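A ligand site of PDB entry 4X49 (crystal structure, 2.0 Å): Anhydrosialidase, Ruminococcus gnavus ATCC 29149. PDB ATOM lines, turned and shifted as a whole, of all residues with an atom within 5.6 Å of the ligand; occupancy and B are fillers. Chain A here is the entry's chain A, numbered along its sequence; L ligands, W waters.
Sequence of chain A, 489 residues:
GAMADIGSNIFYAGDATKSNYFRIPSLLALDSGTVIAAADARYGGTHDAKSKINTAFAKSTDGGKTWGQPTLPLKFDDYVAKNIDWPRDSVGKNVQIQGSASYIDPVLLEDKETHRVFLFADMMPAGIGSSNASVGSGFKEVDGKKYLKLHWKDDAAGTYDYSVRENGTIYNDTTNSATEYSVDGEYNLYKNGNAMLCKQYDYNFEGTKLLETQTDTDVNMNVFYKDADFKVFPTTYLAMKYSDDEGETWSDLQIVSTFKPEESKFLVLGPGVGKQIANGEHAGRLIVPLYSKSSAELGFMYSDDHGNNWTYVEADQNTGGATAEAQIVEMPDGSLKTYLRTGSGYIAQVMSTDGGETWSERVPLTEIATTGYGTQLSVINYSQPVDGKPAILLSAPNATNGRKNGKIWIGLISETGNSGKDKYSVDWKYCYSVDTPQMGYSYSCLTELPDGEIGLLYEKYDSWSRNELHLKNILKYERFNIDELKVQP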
ATOM      1  N   ARG A  23      34.459 -10.566 -28.570  1.00  0.00           N
ATOM      2  CA  ARG A  23      33.395 -11.359 -27.931  1.00  0.00           C
ATOM      3  C   ARG A  23      32.252 -11.566 -28.950  1.00  0.00           C
ATOM      4  O   ARG A  23      32.238 -10.932 -29.997  1.00  0.00           O
ATOM      5  CB  ARG A  23      32.836 -10.621 -26.695  1.00  0.00           C
ATOM      6  CG  ARG A  23      33.570 -10.786 -25.349  1.00  0.00           C
ATOM      7  CD  ARG A  23      32.621 -10.564 -24.168  1.00  0.00           C
ATOM      8  NE  ARG A  23      31.450 -11.429 -24.198  1.00  0.00           N
ATOM      9  CZ  ARG A  23      30.359 -11.364 -23.416  1.00  0.00           C
ATOM     10  NH1 ARG A  23      30.248 -10.435 -22.447  1.00  0.00           N
ATOM     11  NH2 ARG A  23      29.381 -12.275 -23.571  1.00  0.00           N
ATOM     12  N   ILE A  24      31.276 -12.418 -28.565  1.00  0.00           N
ATOM     13  CA  ILE A  24      29.997 -12.609 -29.228  1.00  0.00           C
ATOM     14  C   ILE A  24      30.177 -13.235 -30.629  1.00  0.00           C
ATOM     15  O   ILE A  24      30.025 -12.563 -31.630  1.00  0.00           O
ATOM     16  CB  ILE A  24      29.172 -11.310 -29.337  1.00  0.00           C
ATOM     17  CG1 ILE A  24      29.405 -10.334 -28.193  1.00  0.00           C
ATOM     18  CG2 ILE A  24      27.685 -11.619 -29.514  1.00  0.00           C
ATOM     19  CD1 ILE A  24      29.145 -10.842 -26.762  1.00  0.00           C
ATOM     20  N   ASP A  40      32.158  -9.140 -32.331  1.00  0.00           N
ATOM     21  CA  ASP A  40      32.501  -7.826 -31.865  1.00  0.00           C
ATOM     22  C   ASP A  40      34.011  -7.605 -31.807  1.00  0.00           C
ATOM     23  O   ASP A  40      34.728  -8.450 -31.265  1.00  0.00           O
ATOM     24  CB  ASP A  40      32.060  -7.646 -30.390  1.00  0.00           C
ATOM     25  CG  ASP A  40      30.602  -7.322 -30.203  1.00  0.00           C
ATOM     26  OD1 ASP A  40      29.778  -7.384 -31.101  1.00  0.00           O
ATOM     27  OD2 ASP A  40      30.285  -6.964 -29.042  1.00  0.00           O
ATOM     28  N   ARG A  42      36.065  -5.580 -29.850  1.00  0.00           N
ATOM     29  CA  ARG A  42      35.986  -4.774 -28.656  1.00  0.00           C
ATOM     30  C   ARG A  42      37.369  -4.178 -28.368  1.00  0.00           C
ATOM     31  O   ARG A  42      38.287  -4.844 -27.814  1.00  0.00           O
ATOM     32  CB  ARG A  42      35.439  -5.556 -27.453  1.00  0.00           C
ATOM     33  CG  ARG A  42      34.148  -6.312 -27.734  1.00  0.00           C
ATOM     34  CD  ARG A  42      33.373  -6.676 -26.465  1.00  0.00           C
ATOM     35  NE  ARG A  42      31.950  -6.846 -26.778  1.00  0.00           N
ATOM     36  CZ  ARG A  42      30.976  -7.048 -25.906  1.00  0.00           C
ATOM     37  NH1 ARG A  42      31.239  -7.099 -24.604  1.00  0.00           N
ATOM     38  NH2 ARG A  42      29.744  -7.178 -26.344  1.00  0.00           N
ATOM     39  N   ASP A  48      30.893  -4.591 -22.601  1.00  0.00           N
ATOM     40  CA  ASP A  48      29.709  -4.189 -23.388  1.00  0.00           C
ATOM     41  C   ASP A  48      29.667  -2.676 -23.523  1.00  0.00           C
ATOM     42  O   ASP A  48      30.370  -1.965 -22.821  1.00  0.00           O
ATOM     43  CB  ASP A  48      28.418  -4.688 -22.690  1.00  0.00           C
ATOM     44  CG  ASP A  48      28.277  -6.194 -22.805  1.00  0.00           C
ATOM     45  OD1 ASP A  48      28.553  -6.714 -23.916  1.00  0.00           O
ATOM     46  OD2 ASP A  48      27.901  -6.820 -21.812  1.00  0.00           O
ATOM     47  N   ALA A  49      28.832  -2.222 -24.447  1.00  0.00           N
ATOM     48  CA  ALA A  49      28.607  -0.832 -24.643  1.00  0.00           C
ATOM     49  C   ALA A  49      28.043  -0.303 -23.332  1.00  0.00           C
ATOM     50  O   ALA A  49      27.305  -1.025 -22.658  1.00  0.00           O
ATOM     51  CB  ALA A  49      27.638  -0.622 -25.792  1.00  0.00           C
ATOM     52  N   ILE A 104      27.459  -3.619 -31.702  1.00  0.00           N
ATOM     53  CA  ILE A 104      27.606  -4.693 -30.746  1.00  0.00           C
ATOM     54  C   ILE A 104      26.608  -5.804 -30.979  1.00  0.00           C
ATOM     55  O   ILE A 104      25.479  -5.554 -31.410  1.00  0.00           O
ATOM     56  CB  ILE A 104      27.490  -4.097 -29.324  1.00  0.00           C
ATOM     57  CG1 ILE A 104      27.154  -5.108 -28.253  1.00  0.00           C
ATOM     58  CG2 ILE A 104      26.423  -3.017 -29.256  1.00  0.00           C
ATOM     59  CD1 ILE A 104      27.574  -4.653 -26.875  1.00  0.00           C
ATOM     60  N   ASP A 105      27.050  -7.049 -30.748  1.00  0.00           N
ATOM     61  CA  ASP A 105      26.221  -8.255 -30.749  1.00  0.00           C
ATOM     62  C   ASP A 105      25.688  -8.669 -32.129  1.00  0.00           C
ATOM     63  O   ASP A 105      24.560  -8.390 -32.500  1.00  0.00           O
ATOM     64  CB  ASP A 105      25.061  -8.112 -29.759  1.00  0.00           C
ATOM     65  CG  ASP A 105      25.495  -8.254 -28.296  1.00  0.00           C
ATOM     66  OD1 ASP A 105      26.718  -8.413 -28.025  1.00  0.00           O
ATOM     67  OD2 ASP A 105      24.600  -8.204 -27.398  1.00  0.00           O
ATOM     68  N   ASP A 122      23.366  -4.415 -32.990  1.00  0.00           N
ATOM     69  CA  ASP A 122      22.812  -3.310 -32.234  1.00  0.00           C
ATOM     70  C   ASP A 122      23.654  -2.042 -32.530  1.00  0.00           C
ATOM     71  O   ASP A 122      24.867  -2.144 -32.659  1.00  0.00           O
ATOM     72  CB  ASP A 122      22.934  -3.528 -30.737  1.00  0.00           C
ATOM     73  CG  ASP A 122      22.346  -4.832 -30.252  1.00  0.00           C
ATOM     74  OD1 ASP A 122      21.366  -5.333 -30.860  1.00  0.00           O
ATOM     75  OD2 ASP A 122      22.821  -5.256 -29.162  1.00  0.00           O
ATOM     76  N   MET A 124      24.628   1.655 -31.184  1.00  0.00           N
ATOM     77  CA  MET A 124      24.610   2.514 -30.007  1.00  0.00           C
ATOM     78  C   MET A 124      25.159   3.918 -30.232  1.00  0.00           C
ATOM     79  O   MET A 124      26.337   4.045 -30.514  1.00  0.00           O
ATOM     80  CB  MET A 124      25.479   1.870 -28.913  1.00  0.00           C
ATOM     81  CG  MET A 124      25.099   0.415 -28.511  1.00  0.00           C
ATOM     82  SD  MET A 124      23.445   0.279 -27.779  1.00  0.00           S
ATOM     83  CE  MET A 124      23.577  -1.403 -27.202  1.00  0.00           C
ATOM     84  N   SER A 130      22.910  -0.617 -23.275  1.00  0.00           N
ATOM     85  CA  SER A 130      21.568  -1.034 -22.865  1.00  0.00           C
ATOM     86  C   SER A 130      21.163  -0.312 -21.570  1.00  0.00           C
ATOM     87  O   SER A 130      19.986   0.077 -21.366  1.00  0.00           O
ATOM     88  CB  SER A 130      21.538  -2.578 -22.681  1.00  0.00           C
ATOM     89  OG  SER A 130      22.488  -3.020 -21.694  1.00  0.00           O
ATOM     90  N   PHE A 266      15.477  -0.583 -24.202  1.00  0.00           N
ATOM     91  CA  PHE A 266      16.290  -1.171 -25.208  1.00  0.00           C
ATOM     92  C   PHE A 266      15.536  -2.279 -25.980  1.00  0.00           C
ATOM     93  O   PHE A 266      14.628  -2.913 -25.488  1.00  0.00           O
ATOM     94  CB  PHE A 266      17.602  -1.701 -24.601  1.00  0.00           C
ATOM     95  CG  PHE A 266      17.443  -2.830 -23.618  1.00  0.00           C
ATOM     96  CD1 PHE A 266      17.182  -4.113 -24.057  1.00  0.00           C
ATOM     97  CD2 PHE A 266      17.567  -2.623 -22.256  1.00  0.00           C
ATOM     98  CE1 PHE A 266      17.042  -5.164 -23.146  1.00  0.00           C
ATOM     99  CE2 PHE A 266      17.372  -3.661 -21.355  1.00  0.00           C
ATOM    100  CZ  PHE A 266      17.148  -4.947 -21.809  1.00  0.00           C
ATOM    101  N   VAL A 268      17.219  -5.232 -28.658  1.00  0.00           N
ATOM    102  CA  VAL A 268      18.510  -5.637 -29.133  1.00  0.00           C
ATOM    103  C   VAL A 268      18.434  -7.060 -29.707  1.00  0.00           C
ATOM    104  O   VAL A 268      17.425  -7.771 -29.495  1.00  0.00           O
ATOM    105  CB  VAL A 268      19.513  -5.627 -27.979  1.00  0.00           C
ATOM    106  CG1 VAL A 268      19.770  -4.203 -27.495  1.00  0.00           C
ATOM    107  CG2 VAL A 268      18.992  -6.492 -26.823  1.00  0.00           C
ATOM    108  N   TYR A 291      15.300  -9.230 -28.116  1.00  0.00           N
ATOM    109  CA  TYR A 291      14.725  -9.167 -26.800  1.00  0.00           C
ATOM    110  C   TYR A 291      14.779  -7.702 -26.328  1.00  0.00           C
ATOM    111  O   TYR A 291      15.532  -6.837 -26.925  1.00  0.00           O
ATOM    112  CB  TYR A 291      15.427 -10.135 -25.841  1.00  0.00           C
ATOM    113  CG  TYR A 291      16.870  -9.770 -25.507  1.00  0.00           C
ATOM    114  CD1 TYR A 291      17.929 -10.132 -26.321  1.00  0.00           C
ATOM    115  CD2 TYR A 291      17.159  -9.027 -24.367  1.00  0.00           C
ATOM    116  CE1 TYR A 291      19.232  -9.779 -25.980  1.00  0.00           C
ATOM    117  CE2 TYR A 291      18.442  -8.708 -24.009  1.00  0.00           C
ATOM    118  CZ  TYR A 291      19.491  -9.074 -24.813  1.00  0.00           C
ATOM    119  OH  TYR A 291      20.786  -8.644 -24.473  1.00  0.00           O
ATOM    120  N   THR A 323      17.572 -10.918 -19.908  1.00  0.00           N
ATOM    121  CA  THR A 323      18.458 -11.044 -21.040  1.00  0.00           C
ATOM    122  C   THR A 323      18.029 -12.237 -21.901  1.00  0.00           C
ATOM    123  O   THR A 323      18.678 -13.280 -21.906  1.00  0.00           O
ATOM    124  CB  THR A 323      19.909 -11.165 -20.505  1.00  0.00           C
ATOM    125  OG1 THR A 323      20.227 -10.000 -19.723  1.00  0.00           O
ATOM    126  CG2 THR A 323      20.885 -11.280 -21.634  1.00  0.00           C
ATOM    127  N   GLU A 325      18.106 -13.744 -24.686  1.00  0.00           N
ATOM    128  CA  GLU A 325      18.800 -14.064 -25.926  1.00  0.00           C
ATOM    129  C   GLU A 325      18.358 -15.419 -26.388  1.00  0.00           C
ATOM    130  O   GLU A 325      18.378 -16.397 -25.609  1.00  0.00           O
ATOM    131  CB  GLU A 325      20.310 -14.070 -25.686  1.00  0.00           C
ATOM    132  CG  GLU A 325      20.896 -12.686 -25.297  1.00  0.00           C
ATOM    133  CD  GLU A 325      22.263 -12.857 -24.746  1.00  0.00           C
ATOM    134  OE1 GLU A 325      22.441 -13.891 -24.055  1.00  0.00           O
ATOM    135  OE2 GLU A 325      23.147 -11.982 -25.030  1.00  0.00           O
ATOM    136  N   ARG A 341      17.761 -18.007 -23.317  1.00  0.00           N
ATOM    137  CA  ARG A 341      18.240 -17.646 -22.000  1.00  0.00           C
ATOM    138  C   ARG A 341      17.112 -16.974 -21.248  1.00  0.00           C
ATOM    139  O   ARG A 341      16.273 -16.308 -21.869  1.00  0.00           O
ATOM    140  CB  ARG A 341      19.393 -16.632 -22.211  1.00  0.00           C
ATOM    141  CG  ARG A 341      20.006 -16.029 -20.968  1.00  0.00           C
ATOM    142  CD  ARG A 341      21.248 -15.187 -21.324  1.00  0.00           C
ATOM    143  NE  ARG A 341      21.783 -14.411 -20.242  1.00  0.00           N
ATOM    144  CZ  ARG A 341      22.874 -13.646 -20.316  1.00  0.00           C
ATOM    145  NH1 ARG A 341      23.535 -13.547 -21.467  1.00  0.00           N
ATOM    146  NH2 ARG A 341      23.267 -12.959 -19.267  1.00  0.00           N
ATOM    147  N   GLY A 374      21.936 -16.486 -16.563  1.00  0.00           N
ATOM    148  CA  GLY A 374      22.009 -17.173 -17.836  1.00  0.00           C
ATOM    149  C   GLY A 374      23.197 -16.854 -18.747  1.00  0.00           C
ATOM    150  O   GLY A 374      24.014 -15.954 -18.464  1.00  0.00           O
ATOM    151  N   ARG A 403      30.389 -19.655 -15.799  1.00  0.00           N
ATOM    152  CA  ARG A 403      30.309 -20.004 -17.185  1.00  0.00           C
ATOM    153  C   ARG A 403      31.440 -20.982 -17.529  1.00  0.00           C
ATOM    154  O   ARG A 403      32.625 -20.590 -17.790  1.00  0.00           O
ATOM    155  CB  ARG A 403      30.390 -18.712 -18.026  1.00  0.00           C
ATOM    156  CG  ARG A 403      29.086 -17.926 -18.033  1.00  0.00           C
ATOM    157  CD  ARG A 403      29.102 -16.675 -18.876  1.00  0.00           C
ATOM    158  NE  ARG A 403      27.766 -16.081 -18.960  1.00  0.00           N
ATOM    159  CZ  ARG A 403      27.481 -14.900 -19.504  1.00  0.00           C
ATOM    160  NH1 ARG A 403      28.456 -14.133 -20.031  1.00  0.00           N
ATOM    161  NH2 ARG A 403      26.212 -14.494 -19.533  1.00  0.00           N
ATOM    162  N   TYR A 443      29.625 -17.613 -24.535  1.00  0.00           N
ATOM    163  CA  TYR A 443      28.815 -17.552 -25.719  1.00  0.00           C
ATOM    164  C   TYR A 443      29.446 -18.403 -26.846  1.00  0.00           C
ATOM    165  O   TYR A 443      30.670 -18.614 -26.876  1.00  0.00           O
ATOM    166  CB  TYR A 443      28.714 -16.095 -26.243  1.00  0.00           C
ATOM    167  CG  TYR A 443      27.779 -15.166 -25.481  1.00  0.00           C
ATOM    168  CD1 TYR A 443      27.656 -15.240 -24.133  1.00  0.00           C
ATOM    169  CD2 TYR A 443      27.103 -14.092 -26.149  1.00  0.00           C
ATOM    170  CE1 TYR A 443      26.822 -14.339 -23.452  1.00  0.00           C
ATOM    171  CE2 TYR A 443      26.269 -13.216 -25.470  1.00  0.00           C
ATOM    172  CZ  TYR A 443      26.127 -13.375 -24.130  1.00  0.00           C
ATOM    173  OH  TYR A 443      25.346 -12.570 -23.430  1.00  0.00           O
ATOM    174  N   SER A 463      32.839 -14.937 -19.442  1.00  0.00           N
ATOM    175  CA  SER A 463      32.683 -13.535 -19.921  1.00  0.00           C
ATOM    176  C   SER A 463      31.765 -12.681 -19.058  1.00  0.00           C
ATOM    177  O   SER A 463      31.507 -11.495 -19.339  1.00  0.00           O
ATOM    178  CB  SER A 463      32.211 -13.536 -21.377  1.00  0.00           C
ATOM    179  OG  SER A 463      30.912 -14.116 -21.522  1.00  0.00           O
ATOM    180  N   TRP A 464      31.287 -13.267 -17.989  1.00  0.00           N
ATOM    181  CA  TRP A 464      30.434 -12.605 -16.999  1.00  0.00           C
ATOM    182  C   TRP A 464      31.280 -12.206 -15.839  1.00  0.00           C
ATOM    183  O   TRP A 464      31.162 -11.129 -15.309  1.00  0.00           O
ATOM    184  CB  TRP A 464      29.355 -13.595 -16.499  1.00  0.00           C
ATOM    185  CG  TRP A 464      28.396 -12.959 -15.538  1.00  0.00           C
ATOM    186  CD1 TRP A 464      28.460 -12.966 -14.161  1.00  0.00           C
ATOM    187  CD2 TRP A 464      27.284 -12.142 -15.882  1.00  0.00           C
ATOM    188  NE1 TRP A 464      27.403 -12.216 -13.622  1.00  0.00           N
ATOM    189  CE2 TRP A 464      26.661 -11.727 -14.658  1.00  0.00           C
ATOM    190  CE3 TRP A 464      26.702 -11.765 -17.089  1.00  0.00           C
ATOM    191  CZ2 TRP A 464      25.507 -10.943 -14.625  1.00  0.00           C
ATOM    192  CZ3 TRP A 464      25.564 -10.957 -17.058  1.00  0.00           C
ATOM    193  CH2 TRP A 464      24.987 -10.559 -15.817  1.00  0.00           C
HETATM  194  C1  LIG L   1      26.444 -11.271 -21.156  1.00  0.00           C
HETATM  195  O1  LIG L   1      25.734 -11.915 -20.345  1.00  0.00           O
HETATM  196  O2  LIG L   1      27.679 -11.527 -21.328  1.00  0.00           O
HETATM  197  C2  LIG L   1      25.829 -10.256 -22.008  1.00  0.00           C
HETATM  198  C3  LIG L   1      26.473  -9.954 -23.339  1.00  0.00           C
HETATM  199  C4  LIG L   1      25.641  -9.087 -24.247  1.00  0.00           C
HETATM  200  C5  LIG L   1      24.969  -7.993 -23.437  1.00  0.00           C
HETATM  201  N1  LIG L   1      24.183  -7.154 -24.299  1.00  0.00           N
HETATM  202  C6  LIG L   1      24.368  -5.843 -24.545  1.00  0.00           C
HETATM  203  O3  LIG L   1      25.250  -5.186 -24.030  1.00  0.00           O
HETATM  204  C7  LIG L   1      23.404  -5.246 -25.534  1.00  0.00           C
HETATM  205  C8  LIG L   1      24.051  -8.543 -22.351  1.00  0.00           C
HETATM  206  C9  LIG L   1      24.757  -9.590 -21.572  1.00  0.00           C
HETATM  207  O4  LIG L   1      23.741  -7.461 -21.476  1.00  0.00           O
HETATM  208  C10 LIG L   1      22.468  -7.415 -20.801  1.00  0.00           C
HETATM  209  C11 LIG L   1      22.641  -6.918 -19.360  1.00  0.00           C
HETATM  210  C12 LIG L   1      21.417  -6.409 -21.291  1.00  0.00           C
HETATM  211  C13 LIG L   1      21.450  -6.185 -22.749  1.00  0.00           C
HETATM  212  C14 LIG L   1      23.394  -7.878 -18.462  1.00  0.00           C
HETATM  213  N2  LIG L   1      26.570  -8.523 -25.225  1.00  0.00           N
HETATM  214  O   HOH W   1      25.523  -5.930 -20.459  1.00  0.00           O
HETATM  215  O   HOH W   2      22.687  -9.450 -25.958  1.00  0.00           O
HETATM  216  O   HOH W   3      24.983  -2.237 -23.974  1.00  0.00           O
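Water W1 bridges an oxygen (O4) of the ligand (2.6 Å) and the side-chain carboxylate of Asp 48 (2.9 Å).
Water W3 lies within hydrogen-bond range of N of Ser 130 (2.7 Å), O of Ala 49 (2.9 Å) and O3 of the ligand (3.0 Å).
Water W2 lies within hydrogen-bond range of OH of Tyr 291 (2.5 Å), OD2 of Asp 105 (2.7 Å), OE2 of Glu 325 (2.7 Å) and N1 of the ligand (3.2 Å).
Residues that only touch the ligand: Tyr 291 (3.1 Å), Trp 464 (3.4 Å), Ser 130 (3.5 Å), Thr 323 (3.6 Å), Arg 42 (3.6 Å), Asp 122 (3.7 Å), Ile 104 (3.7 Å), Ile 24 (3.8 Å) and Glu 325 (3.9 Å).
Along chain A the residues within 4 Å of the ligand span positions 23 to 464.
N2 of the ligand lies within salt-bridge range of OD1 of Asp 48 (3.0 Å).
N2 of the ligand lies within salt-bridge range of OD1 of Asp 105, 2.8 Å away.
The side-chain hydroxyl (OH) of Tyr 443 sits close to an oxygen (O1) of the ligand (3.2 Å).
The guanidinium group of Arg 403 is in salt-bridge range of an oxygen (O1) of the ligand, at 2.7 Å.
NH2 of Arg 23 is in salt-bridge range of O2 of the ligand.
NH2 of Arg 341 is in salt-bridge range of O1 of the ligand, at 2.9 Å.
The guanidinium group of Arg 341 sits close to the backbone carbonyl oxygen of Gly 374, 3.2 Å away.
The guanidinium group of Arg 341 lies within hydrogen-bond range of the side-chain hydroxyl of Tyr 443, at 2.8 Å.
N of Val 268 is in hydrogen-bond range of O of Tyr 291 (2.9 Å).
NH1 of Arg 341 is in salt-bridge range of OE1 of Glu 325 (2.8 Å).
The backbone NH of Asp 40 sits at hydrogen-bond distance from the backbone carbonyl oxygen of Arg 23 (2.9 Å).
The side-chain carboxylate of Glu 325 lies within hydrogen-bond range of the side-chain hydroxyl of Tyr 443, at 2.8 Å.
NH2 of Arg 42 lies within salt-bridge range of OD1 of Asp 48, 2.7 Å away.
NH2 of Arg 403 lies within hydrogen-bond range of O of Gly 374, 2.8 Å away.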
